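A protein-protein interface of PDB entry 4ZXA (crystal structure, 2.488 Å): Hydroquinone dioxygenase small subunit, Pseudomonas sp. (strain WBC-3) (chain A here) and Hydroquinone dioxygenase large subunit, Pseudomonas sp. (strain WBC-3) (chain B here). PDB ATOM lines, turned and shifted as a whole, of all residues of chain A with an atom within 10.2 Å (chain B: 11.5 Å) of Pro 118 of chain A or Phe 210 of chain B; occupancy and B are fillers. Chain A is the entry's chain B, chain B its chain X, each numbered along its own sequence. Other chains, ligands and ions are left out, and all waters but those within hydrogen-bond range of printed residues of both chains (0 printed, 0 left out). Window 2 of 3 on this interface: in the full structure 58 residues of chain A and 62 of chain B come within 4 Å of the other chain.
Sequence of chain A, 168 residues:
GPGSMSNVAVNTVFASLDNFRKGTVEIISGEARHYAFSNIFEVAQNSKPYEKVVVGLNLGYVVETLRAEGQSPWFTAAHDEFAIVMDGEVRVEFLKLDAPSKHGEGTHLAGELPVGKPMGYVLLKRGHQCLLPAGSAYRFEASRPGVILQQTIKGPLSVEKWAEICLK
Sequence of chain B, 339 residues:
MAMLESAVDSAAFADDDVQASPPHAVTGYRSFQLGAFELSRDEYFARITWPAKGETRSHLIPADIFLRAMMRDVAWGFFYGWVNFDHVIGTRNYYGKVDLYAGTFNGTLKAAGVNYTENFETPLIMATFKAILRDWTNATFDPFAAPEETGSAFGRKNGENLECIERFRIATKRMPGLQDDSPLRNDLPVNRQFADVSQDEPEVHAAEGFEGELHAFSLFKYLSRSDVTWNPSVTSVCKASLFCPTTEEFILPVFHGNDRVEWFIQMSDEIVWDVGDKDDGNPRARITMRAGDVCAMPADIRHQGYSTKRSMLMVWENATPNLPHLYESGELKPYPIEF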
ATOM      1  N   TRP A  74      20.077   8.775  -9.557  1.00  0.00           N
ATOM      2  CA  TRP A  74      19.432   9.308  -8.368  1.00  0.00           C
ATOM      3  C   TRP A  74      17.922   9.211  -8.534  1.00  0.00           C
ATOM      4  O   TRP A  74      17.376   9.593  -9.570  1.00  0.00           O
ATOM      5  CB  TRP A  74      19.813  10.767  -8.158  1.00  0.00           C
ATOM      6  CG  TRP A  74      21.173  10.990  -7.584  1.00  0.00           C
ATOM      7  CD1 TRP A  74      22.307  11.348  -8.264  1.00  0.00           C
ATOM      8  CD2 TRP A  74      21.546  10.899  -6.205  1.00  0.00           C
ATOM      9  NE1 TRP A  74      23.358  11.479  -7.394  1.00  0.00           N
ATOM     10  CE2 TRP A  74      22.920  11.214  -6.124  1.00  0.00           C
ATOM     11  CE3 TRP A  74      20.853  10.581  -5.031  1.00  0.00           C
ATOM     12  CZ2 TRP A  74      23.616  11.217  -4.914  1.00  0.00           C
ATOM     13  CZ3 TRP A  74      21.545  10.591  -3.831  1.00  0.00           C
ATOM     14  CH2 TRP A  74      22.916  10.903  -3.784  1.00  0.00           C
ATOM     15  N   ARG A  91      24.664  -0.471  -1.193  1.00  0.00           N
ATOM     16  CA  ARG A  91      24.883   0.740  -0.431  1.00  0.00           C
ATOM     17  C   ARG A  91      23.934   1.804  -0.973  1.00  0.00           C
ATOM     18  O   ARG A  91      23.857   2.022  -2.193  1.00  0.00           O
ATOM     19  CB  ARG A  91      26.345   1.159  -0.572  1.00  0.00           C
ATOM     20  CG  ARG A  91      26.627   2.644  -0.516  1.00  0.00           C
ATOM     21  CD  ARG A  91      28.058   2.915  -0.985  1.00  0.00           C
ATOM     22  NE  ARG A  91      28.725   3.863  -0.102  1.00  0.00           N
ATOM     23  CZ  ARG A  91      28.670   5.181  -0.255  1.00  0.00           C
ATOM     24  NH1 ARG A  91      27.992   5.703  -1.270  1.00  0.00           N
ATOM     25  NH2 ARG A  91      29.291   5.977   0.609  1.00  0.00           N
ATOM     26  N   VAL A  92      23.192   2.440  -0.066  1.00  0.00           N
ATOM     27  CA  VAL A  92      22.199   3.440  -0.451  1.00  0.00           C
ATOM     28  C   VAL A  92      22.606   4.820   0.057  1.00  0.00           C
ATOM     29  O   VAL A  92      22.740   5.036   1.267  1.00  0.00           O
ATOM     30  CB  VAL A  92      20.779   3.085   0.082  1.00  0.00           C
ATOM     31  CG1 VAL A  92      19.726   3.973  -0.562  1.00  0.00           C
ATOM     32  CG2 VAL A  92      20.460   1.632  -0.186  1.00  0.00           C
ATOM     33  N   GLU A  93      22.813   5.746  -0.877  1.00  0.00           N
ATOM     34  CA  GLU A  93      23.172   7.117  -0.533  1.00  0.00           C
ATOM     35  C   GLU A  93      21.922   7.979  -0.452  1.00  0.00           C
ATOM     36  O   GLU A  93      21.047   7.883  -1.314  1.00  0.00           O
ATOM     37  CB  GLU A  93      24.098   7.721  -1.587  1.00  0.00           C
ATOM     38  CG  GLU A  93      25.541   7.274  -1.538  1.00  0.00           C
ATOM     39  CD  GLU A  93      26.338   7.841  -2.699  1.00  0.00           C
ATOM     40  OE1 GLU A  93      26.714   9.036  -2.633  1.00  0.00           O
ATOM     41  OE2 GLU A  93      26.564   7.101  -3.687  1.00  0.00           O
ATOM     42  N   PHE A  94      21.859   8.836   0.567  1.00  0.00           N
ATOM     43  CA  PHE A  94      20.726   9.735   0.754  1.00  0.00           C
ATOM     44  C   PHE A  94      21.089  11.218   0.647  1.00  0.00           C
ATOM     45  O   PHE A  94      22.171  11.651   1.043  1.00  0.00           O
ATOM     46  CB  PHE A  94      20.053   9.467   2.094  1.00  0.00           C
ATOM     47  CG  PHE A  94      19.449   8.105   2.199  1.00  0.00           C
ATOM     48  CD1 PHE A  94      18.130   7.891   1.831  1.00  0.00           C
ATOM     49  CD2 PHE A  94      20.200   7.034   2.655  1.00  0.00           C
ATOM     50  CE1 PHE A  94      17.566   6.638   1.919  1.00  0.00           C
ATOM     51  CE2 PHE A  94      19.644   5.777   2.755  1.00  0.00           C
ATOM     52  CZ  PHE A  94      18.323   5.577   2.386  1.00  0.00           C
ATOM     53  N   LEU A  95      20.144  11.989   0.127  1.00  0.00           N
ATOM     54  CA  LEU A  95      20.330  13.403  -0.131  1.00  0.00           C
ATOM     55  C   LEU A  95      19.061  14.145   0.276  1.00  0.00           C
ATOM     56  O   LEU A  95      17.998  13.924  -0.304  1.00  0.00           O
ATOM     57  CB  LEU A  95      20.580  13.609  -1.631  1.00  0.00           C
ATOM     58  CG  LEU A  95      21.862  14.305  -2.103  1.00  0.00           C
ATOM     59  CD1 LEU A  95      21.624  15.791  -2.367  1.00  0.00           C
ATOM     60  CD2 LEU A  95      23.022  14.077  -1.122  1.00  0.00           C
ATOM     61  N   LYS A  96      19.159  15.017   1.270  1.00  0.00           N
ATOM     62  CA  LYS A  96      17.999  15.804   1.662  1.00  0.00           C
ATOM     63  C   LYS A  96      17.833  17.011   0.741  1.00  0.00           C
ATOM     64  O   LYS A  96      18.467  18.043   0.947  1.00  0.00           O
ATOM     65  CB  LYS A  96      18.119  16.257   3.113  1.00  0.00           C
ATOM     66  CG  LYS A  96      16.922  17.066   3.585  1.00  0.00           C
ATOM     67  CD  LYS A  96      16.923  17.278   5.098  1.00  0.00           C
ATOM     68  CE  LYS A  96      15.768  18.182   5.536  1.00  0.00           C
ATOM     69  NZ  LYS A  96      15.978  18.734   6.913  1.00  0.00           N
ATOM     70  N   LEU A  97      16.978  16.879  -0.270  1.00  0.00           N
ATOM     71  CA  LEU A  97      16.786  17.938  -1.264  1.00  0.00           C
ATOM     72  C   LEU A  97      16.243  19.236  -0.665  1.00  0.00           C
ATOM     73  O   LEU A  97      15.467  19.214   0.293  1.00  0.00           O
ATOM     74  CB  LEU A  97      15.860  17.478  -2.390  1.00  0.00           C
ATOM     75  CG  LEU A  97      16.316  16.338  -3.300  1.00  0.00           C
ATOM     76  CD1 LEU A  97      15.284  16.079  -4.389  1.00  0.00           C
ATOM     77  CD2 LEU A  97      17.659  16.645  -3.914  1.00  0.00           C
ATOM     78  N   ASP A  98      16.655  20.362  -1.246  1.00  0.00           N
ATOM     79  CA  ASP A  98      16.207  21.681  -0.808  1.00  0.00           C
ATOM     80  C   ASP A  98      14.799  21.955  -1.326  1.00  0.00           C
ATOM     81  O   ASP A  98      14.026  22.672  -0.682  1.00  0.00           O
ATOM     82  CB  ASP A  98      17.174  22.788  -1.278  1.00  0.00           C
ATOM     83  CG  ASP A  98      18.548  22.712  -0.598  1.00  0.00           C
ATOM     84  OD1 ASP A  98      18.628  22.249   0.561  1.00  0.00           O
ATOM     85  OD2 ASP A  98      19.553  23.117  -1.223  1.00  0.00           O
ATOM     86  N   PRO A 114      21.720  16.434  -8.101  1.00  0.00           N
ATOM     87  CA  PRO A 114      20.639  16.816  -7.186  1.00  0.00           C
ATOM     88  C   PRO A 114      21.127  17.852  -6.191  1.00  0.00           C
ATOM     89  O   PRO A 114      22.285  17.798  -5.766  1.00  0.00           O
ATOM     90  CB  PRO A 114      20.302  15.504  -6.466  1.00  0.00           C
ATOM     91  CG  PRO A 114      20.876  14.414  -7.343  1.00  0.00           C
ATOM     92  CD  PRO A 114      22.098  15.018  -7.954  1.00  0.00           C
ATOM     93  N   VAL A 115      20.252  18.784  -5.831  1.00  0.00           N
ATOM     94  CA  VAL A 115      20.623  19.884  -4.957  1.00  0.00           C
ATOM     95  C   VAL A 115      20.153  19.644  -3.541  1.00  0.00           C
ATOM     96  O   VAL A 115      18.953  19.606  -3.293  1.00  0.00           O
ATOM     97  CB  VAL A 115      19.987  21.208  -5.428  1.00  0.00           C
ATOM     98  CG1 VAL A 115      20.170  22.313  -4.356  1.00  0.00           C
ATOM     99  CG2 VAL A 115      20.556  21.627  -6.784  1.00  0.00           C
ATOM    100  N   GLY A 116      21.089  19.506  -2.609  1.00  0.00           N
ATOM    101  CA  GLY A 116      20.728  19.325  -1.215  1.00  0.00           C
ATOM    102  C   GLY A 116      21.861  18.787  -0.370  1.00  0.00           C
ATOM    103  O   GLY A 116      22.916  18.449  -0.887  1.00  0.00           O
ATOM    104  N   LYS A 117      21.634  18.702   0.935  1.00  0.00           N
ATOM    105  CA  LYS A 117      22.662  18.260   1.868  1.00  0.00           C
ATOM    106  C   LYS A 117      22.742  16.731   1.957  1.00  0.00           C
ATOM    107  O   LYS A 117      21.721  16.056   2.085  1.00  0.00           O
ATOM    108  CB  LYS A 117      22.391  18.851   3.256  1.00  0.00           C
ATOM    109  CG  LYS A 117      21.869  20.278   3.220  1.00  0.00           C
ATOM    110  CD  LYS A 117      21.976  20.964   4.575  1.00  0.00           C
ATOM    111  CE  LYS A 117      21.598  22.431   4.460  1.00  0.00           C
ATOM    112  NZ  LYS A 117      22.289  23.081   3.302  1.00  0.00           N
ATOM    113  N   PRO A 118      23.961  16.177   1.879  1.00  0.00           N
ATOM    114  CA  PRO A 118      24.137  14.741   2.121  1.00  0.00           C
ATOM    115  C   PRO A 118      23.625  14.351   3.508  1.00  0.00           C
ATOM    116  O   PRO A 118      23.776  15.125   4.463  1.00  0.00           O
ATOM    117  CB  PRO A 118      25.655  14.565   2.047  1.00  0.00           C
ATOM    118  CG  PRO A 118      26.114  15.669   1.134  1.00  0.00           C
ATOM    119  CD  PRO A 118      25.212  16.830   1.451  1.00  0.00           C
ATOM    120  N   MET A 119      23.022  13.167   3.617  1.00  0.00           N
ATOM    121  CA  MET A 119      22.469  12.703   4.888  1.00  0.00           C
ATOM    122  C   MET A 119      23.287  11.543   5.448  1.00  0.00           C
ATOM    123  O   MET A 119      23.171  11.188   6.625  1.00  0.00           O
ATOM    124  CB  MET A 119      21.016  12.271   4.701  1.00  0.00           C
ATOM    125  CG  MET A 119      20.167  13.269   3.939  1.00  0.00           C
ATOM    126  SD  MET A 119      18.445  12.748   3.818  1.00  0.00           S
ATOM    127  CE  MET A 119      17.989  12.611   5.551  1.00  0.00           C
ATOM    128  N   GLY A 120      24.119  10.964   4.588  1.00  0.00           N
ATOM    129  CA  GLY A 120      24.909   9.803   4.937  1.00  0.00           C
ATOM    130  C   GLY A 120      24.532   8.646   4.035  1.00  0.00           C
ATOM    131  O   GLY A 120      23.839   8.821   3.029  1.00  0.00           O
ATOM    132  N   TYR A 121      24.985   7.451   4.389  1.00  0.00           N
ATOM    133  CA  TYR A 121      24.625   6.273   3.618  1.00  0.00           C
ATOM    134  C   TYR A 121      24.236   5.117   4.527  1.00  0.00           C
ATOM    135  O   TYR A 121      24.408   5.185   5.751  1.00  0.00           O
ATOM    136  CB  TYR A 121      25.767   5.869   2.681  1.00  0.00           C
ATOM    137  CG  TYR A 121      27.042   5.474   3.392  1.00  0.00           C
ATOM    138  CD1 TYR A 121      27.945   6.438   3.828  1.00  0.00           C
ATOM    139  CD2 TYR A 121      27.347   4.135   3.622  1.00  0.00           C
ATOM    140  CE1 TYR A 121      29.110   6.081   4.481  1.00  0.00           C
ATOM    141  CE2 TYR A 121      28.513   3.768   4.269  1.00  0.00           C
ATOM    142  CZ  TYR A 121      29.391   4.745   4.700  1.00  0.00           C
ATOM    143  OH  TYR A 121      30.555   4.388   5.346  1.00  0.00           O
ATOM    144  N   VAL A 122      23.686   4.069   3.924  1.00  0.00           N
ATOM    145  CA  VAL A 122      23.354   2.855   4.650  1.00  0.00           C
ATOM    146  C   VAL A 122      23.889   1.658   3.878  1.00  0.00           C
ATOM    147  O   VAL A 122      23.904   1.671   2.646  1.00  0.00           O
ATOM    148  CB  VAL A 122      21.827   2.715   4.866  1.00  0.00           C
ATOM    149  CG1 VAL A 122      21.487   1.314   5.310  1.00  0.00           C
ATOM    150  CG2 VAL A 122      21.336   3.718   5.895  1.00  0.00           C
ATOM    151  N   PRO A 133      13.050   7.775   2.598  1.00  0.00           N
ATOM    152  CA  PRO A 133      12.182   8.838   3.123  1.00  0.00           C
ATOM    153  C   PRO A 133      11.710   9.810   2.049  1.00  0.00           C
ATOM    154  O   PRO A 133      12.499  10.275   1.220  1.00  0.00           O
ATOM    155  CB  PRO A 133      13.072   9.569   4.145  1.00  0.00           C
ATOM    156  CG  PRO A 133      14.299   8.732   4.296  1.00  0.00           C
ATOM    157  CD  PRO A 133      14.445   7.957   3.021  1.00  0.00           C
ATOM    158  N   GLY A 135      10.874  12.880  -0.029  1.00  0.00           N
ATOM    159  CA  GLY A 135      11.480  14.186  -0.174  1.00  0.00           C
ATOM    160  C   GLY A 135      12.990  14.106  -0.109  1.00  0.00           C
ATOM    161  O   GLY A 135      13.687  15.131  -0.076  1.00  0.00           O
ATOM    162  N   SER A 136      13.505  12.884  -0.079  1.00  0.00           N
ATOM    163  CA  SER A 136      14.939  12.690  -0.192  1.00  0.00           C
ATOM    164  C   SER A 136      15.251  12.171  -1.586  1.00  0.00           C
ATOM    165  O   SER A 136      14.352  11.739  -2.304  1.00  0.00           O
ATOM    166  CB  SER A 136      15.426  11.694   0.854  1.00  0.00           C
ATOM    167  OG  SER A 136      15.199  10.362   0.426  1.00  0.00           O
ATOM    168  N   ALA A 137      16.518  12.224  -1.979  1.00  0.00           N
ATOM    169  CA  ALA A 137      16.948  11.511  -3.173  1.00  0.00           C
ATOM    170  C   ALA A 137      17.928  10.456  -2.712  1.00  0.00           C
ATOM    171  O   ALA A 137      18.563  10.607  -1.667  1.00  0.00           O
ATOM    172  CB  ALA A 137      17.584  12.442  -4.160  1.00  0.00           C
ATOM    173  N   TYR A 138      18.047   9.381  -3.473  1.00  0.00           N
ATOM    174  CA  TYR A 138      18.810   8.231  -3.012  1.00  0.00           C
ATOM    175  C   TYR A 138      19.333   7.451  -4.207  1.00  0.00           C
ATOM    176  O   TYR A 138      18.759   7.519  -5.299  1.00  0.00           O
ATOM    177  CB  TYR A 138      17.924   7.327  -2.138  1.00  0.00           C
ATOM    178  CG  TYR A 138      16.672   6.832  -2.850  1.00  0.00           C
ATOM    179  CD1 TYR A 138      15.433   7.421  -2.615  1.00  0.00           C
ATOM    180  CD2 TYR A 138      16.738   5.801  -3.779  1.00  0.00           C
ATOM    181  CE1 TYR A 138      14.288   6.983  -3.271  1.00  0.00           C
ATOM    182  CE2 TYR A 138      15.607   5.359  -4.444  1.00  0.00           C
ATOM    183  CZ  TYR A 138      14.384   5.949  -4.181  1.00  0.00           C
ATOM    184  OH  TYR A 138      13.255   5.502  -4.834  1.00  0.00           O
ATOM    185  N   ARG A 139      20.421   6.718  -4.016  1.00  0.00           N
ATOM    186  CA  ARG A 139      20.902   5.854  -5.087  1.00  0.00           C
ATOM    187  C   ARG A 139      21.596   4.619  -4.556  1.00  0.00           C
ATOM    188  O   ARG A 139      22.050   4.582  -3.417  1.00  0.00           O
ATOM    189  CB  ARG A 139      21.805   6.604  -6.067  1.00  0.00           C
ATOM    190  CG  ARG A 139      23.241   6.792  -5.604  1.00  0.00           C
ATOM    191  CD  ARG A 139      24.095   7.322  -6.744  1.00  0.00           C
ATOM    192  NE  ARG A 139      24.972   8.395  -6.295  1.00  0.00           N
ATOM    193  CZ  ARG A 139      25.713   9.142  -7.105  1.00  0.00           C
ATOM    194  NH1 ARG A 139      25.696   8.938  -8.419  1.00  0.00           N
ATOM    195  NH2 ARG A 139      26.473  10.096  -6.596  1.00  0.00           N
ATOM    196  N   GLN B 179      11.421   6.194  15.810  1.00  0.00           N
ATOM    197  CA  GLN B 179      11.028   6.908  17.013  1.00  0.00           C
ATOM    198  C   GLN B 179       9.516   6.828  17.232  1.00  0.00           C
ATOM    199  O   GLN B 179       8.735   7.219  16.363  1.00  0.00           O
ATOM    200  CB  GLN B 179      11.469   8.374  16.910  1.00  0.00           C
ATOM    201  CG  GLN B 179      12.706   8.709  17.721  1.00  0.00           C
ATOM    202  CD  GLN B 179      12.483   8.504  19.210  1.00  0.00           C
ATOM    203  OE1 GLN B 179      13.222   7.767  19.869  1.00  0.00           O
ATOM    204  NE2 GLN B 179      11.454   9.157  19.747  1.00  0.00           N
ATOM    205  N   VAL B 204      24.393   1.745   9.459  1.00  0.00           N
ATOM    206  CA  VAL B 204      23.862   3.071   9.173  1.00  0.00           C
ATOM    207  C   VAL B 204      24.910   4.148   9.471  1.00  0.00           C
ATOM    208  O   VAL B 204      25.167   4.471  10.633  1.00  0.00           O
ATOM    209  CB  VAL B 204      22.595   3.355  10.000  1.00  0.00           C
ATOM    210  CG1 VAL B 204      21.999   4.706   9.623  1.00  0.00           C
ATOM    211  CG2 VAL B 204      21.579   2.234   9.809  1.00  0.00           C
ATOM    212  N   HIS B 205      25.516   4.685   8.415  1.00  0.00           N
ATOM    213  CA  HIS B 205      26.507   5.751   8.538  1.00  0.00           C
ATOM    214  C   HIS B 205      25.882   7.111   8.241  1.00  0.00           C
ATOM    215  O   HIS B 205      25.876   7.568   7.094  1.00  0.00           O
ATOM    216  CB  HIS B 205      27.697   5.499   7.610  1.00  0.00           C
ATOM    217  CG  HIS B 205      28.472   4.264   7.948  1.00  0.00           C
ATOM    218  ND1 HIS B 205      29.093   4.086   9.165  1.00  0.00           N
ATOM    219  CD2 HIS B 205      28.723   3.143   7.230  1.00  0.00           C
ATOM    220  CE1 HIS B 205      29.695   2.910   9.183  1.00  0.00           C
ATOM    221  NE2 HIS B 205      29.488   2.318   8.020  1.00  0.00           N
ATOM    222  N   ALA B 206      25.354   7.747   9.281  1.00  0.00           N
ATOM    223  CA  ALA B 206      24.751   9.072   9.163  1.00  0.00           C
ATOM    224  C   ALA B 206      25.812  10.170   9.098  1.00  0.00           C
ATOM    225  O   ALA B 206      26.857  10.085   9.753  1.00  0.00           O
ATOM    226  CB  ALA B 206      23.813   9.331  10.331  1.00  0.00           C
ATOM    227  N   ALA B 207      25.536  11.203   8.308  1.00  0.00           N
ATOM    228  CA  ALA B 207      26.445  12.336   8.199  1.00  0.00           C
ATOM    229  C   ALA B 207      26.129  13.361   9.280  1.00  0.00           C
ATOM    230  O   ALA B 207      24.998  13.832   9.381  1.00  0.00           O
ATOM    231  CB  ALA B 207      26.353  12.961   6.819  1.00  0.00           C
ATOM    232  N   GLU B 208      27.136  13.700  10.082  1.00  0.00           N
ATOM    233  CA  GLU B 208      26.954  14.588  11.230  1.00  0.00           C
ATOM    234  C   GLU B 208      25.915  15.684  10.969  1.00  0.00           C
ATOM    235  O   GLU B 208      25.976  16.393   9.961  1.00  0.00           O
ATOM    236  CB  GLU B 208      28.295  15.190  11.672  1.00  0.00           C
ATOM    237  CG  GLU B 208      29.328  14.163  12.162  1.00  0.00           C
ATOM    238  CD  GLU B 208      29.117  13.730  13.616  1.00  0.00           C
ATOM    239  OE1 GLU B 208      28.238  14.307  14.297  1.00  0.00           O
ATOM    240  OE2 GLU B 208      29.838  12.812  14.076  1.00  0.00           O
ATOM    241  N   GLY B 209      24.958  15.802  11.887  1.00  0.00           N
ATOM    242  CA  GLY B 209      23.849  16.728  11.738  1.00  0.00           C
ATOM    243  C   GLY B 209      22.604  16.023  11.227  1.00  0.00           C
ATOM    244  O   GLY B 209      21.580  16.652  10.947  1.00  0.00           O
ATOM    245  N   PHE B 210      22.691  14.703  11.108  1.00  0.00           N
ATOM    246  CA  PHE B 210      21.616  13.925  10.518  1.00  0.00           C
ATOM    247  C   PHE B 210      21.404  12.609  11.240  1.00  0.00           C
ATOM    248  O   PHE B 210      20.779  11.699  10.700  1.00  0.00           O
ATOM    249  CB  PHE B 210      21.912  13.651   9.045  1.00  0.00           C
ATOM    250  CG  PHE B 210      21.387  14.706   8.112  1.00  0.00           C
ATOM    251  CD1 PHE B 210      22.231  15.669   7.583  1.00  0.00           C
ATOM    252  CD2 PHE B 210      20.044  14.732   7.764  1.00  0.00           C
ATOM    253  CE1 PHE B 210      21.747  16.635   6.725  1.00  0.00           C
ATOM    254  CE2 PHE B 210      19.551  15.697   6.907  1.00  0.00           C
ATOM    255  CZ  PHE B 210      20.406  16.649   6.386  1.00  0.00           C
ATOM    256  N   GLU B 211      21.925  12.504  12.456  1.00  0.00           N
ATOM    257  CA  GLU B 211      21.785  11.274  13.226  1.00  0.00           C
ATOM    258  C   GLU B 211      20.305  10.947  13.392  1.00  0.00           C
ATOM    259  O   GLU B 211      19.474  11.846  13.559  1.00  0.00           O
ATOM    260  CB  GLU B 211      22.464  11.394  14.597  1.00  0.00           C
ATOM    261  CG  GLU B 211      23.671  12.339  14.643  1.00  0.00           C
ATOM    262  CD  GLU B 211      24.846  11.886  13.779  1.00  0.00           C
ATOM    263  OE1 GLU B 211      24.806  10.759  13.228  1.00  0.00           O
ATOM    264  OE2 GLU B 211      25.818  12.666  13.654  1.00  0.00           O
ATOM    265  N   GLY B 212      19.979   9.661  13.324  1.00  0.00           N
ATOM    266  CA  GLY B 212      18.610   9.214  13.507  1.00  0.00           C
ATOM    267  C   GLY B 212      17.638   9.744  12.466  1.00  0.00           C
ATOM    268  O   GLY B 212      16.435   9.839  12.725  1.00  0.00           O
ATOM    269  N   GLU B 213      18.153  10.098  11.291  1.00  0.00           N
ATOM    270  CA  GLU B 213      17.305  10.503  10.170  1.00  0.00           C
ATOM    271  C   GLU B 213      17.306   9.412   9.109  1.00  0.00           C
ATOM    272  O   GLU B 213      16.519   9.440   8.159  1.00  0.00           O
ATOM    273  CB  GLU B 213      17.795  11.819   9.559  1.00  0.00           C
ATOM    274  CG  GLU B 213      17.747  13.004  10.504  1.00  0.00           C
ATOM    275  CD  GLU B 213      16.335  13.513  10.732  1.00  0.00           C
ATOM    276  OE1 GLU B 213      15.551  13.575   9.755  1.00  0.00           O
ATOM    277  OE2 GLU B 213      16.014  13.851  11.895  1.00  0.00           O
ATOM    278  N   LEU B 214      18.218   8.462   9.265  1.00  0.00           N
ATOM    279  CA  LEU B 214      18.255   7.295   8.405  1.00  0.00           C
ATOM    280  C   LEU B 214      17.847   6.066   9.215  1.00  0.00           C
ATOM    281  O   LEU B 214      18.173   5.958  10.404  1.00  0.00           O
ATOM    282  CB  LEU B 214      19.637   7.133   7.771  1.00  0.00           C
ATOM    283  CG  LEU B 214      19.994   8.227   6.762  1.00  0.00           C
ATOM    284  CD1 LEU B 214      21.207   7.822   5.940  1.00  0.00           C
ATOM    285  CD2 LEU B 214      18.814   8.540   5.844  1.00  0.00           C
ATOM    286  N   HIS B 215      17.112   5.160   8.575  1.00  0.00           N
ATOM    287  CA  HIS B 215      16.488   4.034   9.277  1.00  0.00           C
ATOM    288  C   HIS B 215      16.567   2.731   8.474  1.00  0.00           C
ATOM    289  O   HIS B 215      16.199   2.662   7.289  1.00  0.00           O
ATOM    290  CB  HIS B 215      15.038   4.366   9.598  1.00  0.00           C
ATOM    291  CG  HIS B 215      14.864   5.629  10.380  1.00  0.00           C
ATOM    292  ND1 HIS B 215      15.030   5.689  11.750  1.00  0.00           N
ATOM    293  CD2 HIS B 215      14.523   6.880   9.987  1.00  0.00           C
ATOM    294  CE1 HIS B 215      14.797   6.922  12.167  1.00  0.00           C
ATOM    295  NE2 HIS B 215      14.491   7.665  11.117  1.00  0.00           N
ATOM    296  N   ALA B 216      17.064   1.692   9.122  1.00  0.00           N
ATOM    297  CA  ALA B 216      17.265   0.430   8.438  1.00  0.00           C
ATOM    298  C   ALA B 216      17.461  -0.651   9.471  1.00  0.00           C
ATOM    299  O   ALA B 216      18.098  -0.421  10.496  1.00  0.00           O
ATOM    300  CB  ALA B 216      18.471   0.510   7.503  1.00  0.00           C
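The backbone carbonyl oxygen (O) of Met 119 of chain A sits at hydrogen-bond distance from the backbone NH (N) of Ala 207 of chain B, at 2.9 Å. O of His 205 of chain B lies within hydrogen-bond range of N of Tyr 121 of chain A (2.9 Å).
N of Lys 96 of chain A lies within hydrogen-bond range of O of Lys 117 of chain A (2.9 Å). The backbone NH of Met 119 of chain A sits at hydrogen-bond distance from the backbone carbonyl oxygen of Phe 94 of chain A. The side-chain sulfur of Met 119 of chain A sits close to the backbone NH of Lys 96 of chain A, at 3.5 Å. N of Phe 94 of chain A is in hydrogen-bond range of O of Gly 120 of chain A (3.2 Å).
Among the printed residues, pairs that only touch across the chains: Phe 94 of chain A with Leu 214 of chain B, Lys 96 of chain A with Phe 210 of chain B, Pro 118 of chain A with Phe 210 of chain B, Met 119 of chain A with Ala 206 of chain B, Met 119 of chain A with Phe 210 of chain B, Met 119 of chain A with Leu 214 of chain B, Gly 120 of chain A with His 205 of chain B, Gly 120 of chain A with Ala 207 of chain B, Gly 120 of chain A with Leu 214 of chain B, Tyr 121 of chain A with Val 204 of chain B, Val 122 of chain A with Val 204 of chain B and Val 122 of chain A with Ala 216 of chain B.
Pro 118 of chain A touches just one residue of chain B: Phe 210. Of chain A, only Lys 96, Pro 118 and Met 119 come within 4 Å of Phe 210 of chain B. Leu 95 of chain A touches none of the printed residues of chain B. Of chain A, only Met 119 (2.9 Å) and Gly 120 (3.7 Å) come within 4 Å of Ala 207 of chain B. No residue of chain A comes within 4 Å of Gly 209 of chain B. No residue of chain A comes within 4 Å of Gly 212 of chain B. Of the printed residues of chain A, Leu 214 of chain B touches Phe 94, Met 119 and Gly 120. Of the printed residues of chain B, Tyr 121 of chain A touches Val 204 and His 205. Printed residues of chain A within 4 Å of Val 204 of chain B: Tyr 121 and Val 122. Of the printed residues of chain A, Ala 216 of chain B touches Val 122. The nearest residue of chain A that does not touch Phe 210 of chain B is Lys 117 of chain A (4.2 Å).
Of the 14 printed residues of chain B, 7 touch a printed residue of chain A. Printed residues of chain B that touch a printed residue of chain A: Val 204, His 205, Ala 206, Ala 207, Phe 210, Leu 214 and Ala 216. Hydrophobic or aromatic side chains of chain B within 4 Å of the printed part of chain A: Val 204, His 205, Ala 207, Phe 210, Leu 214 and Ala 216. Of the 24 printed residues of chain A, 7 touch a printed residue of chain B.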
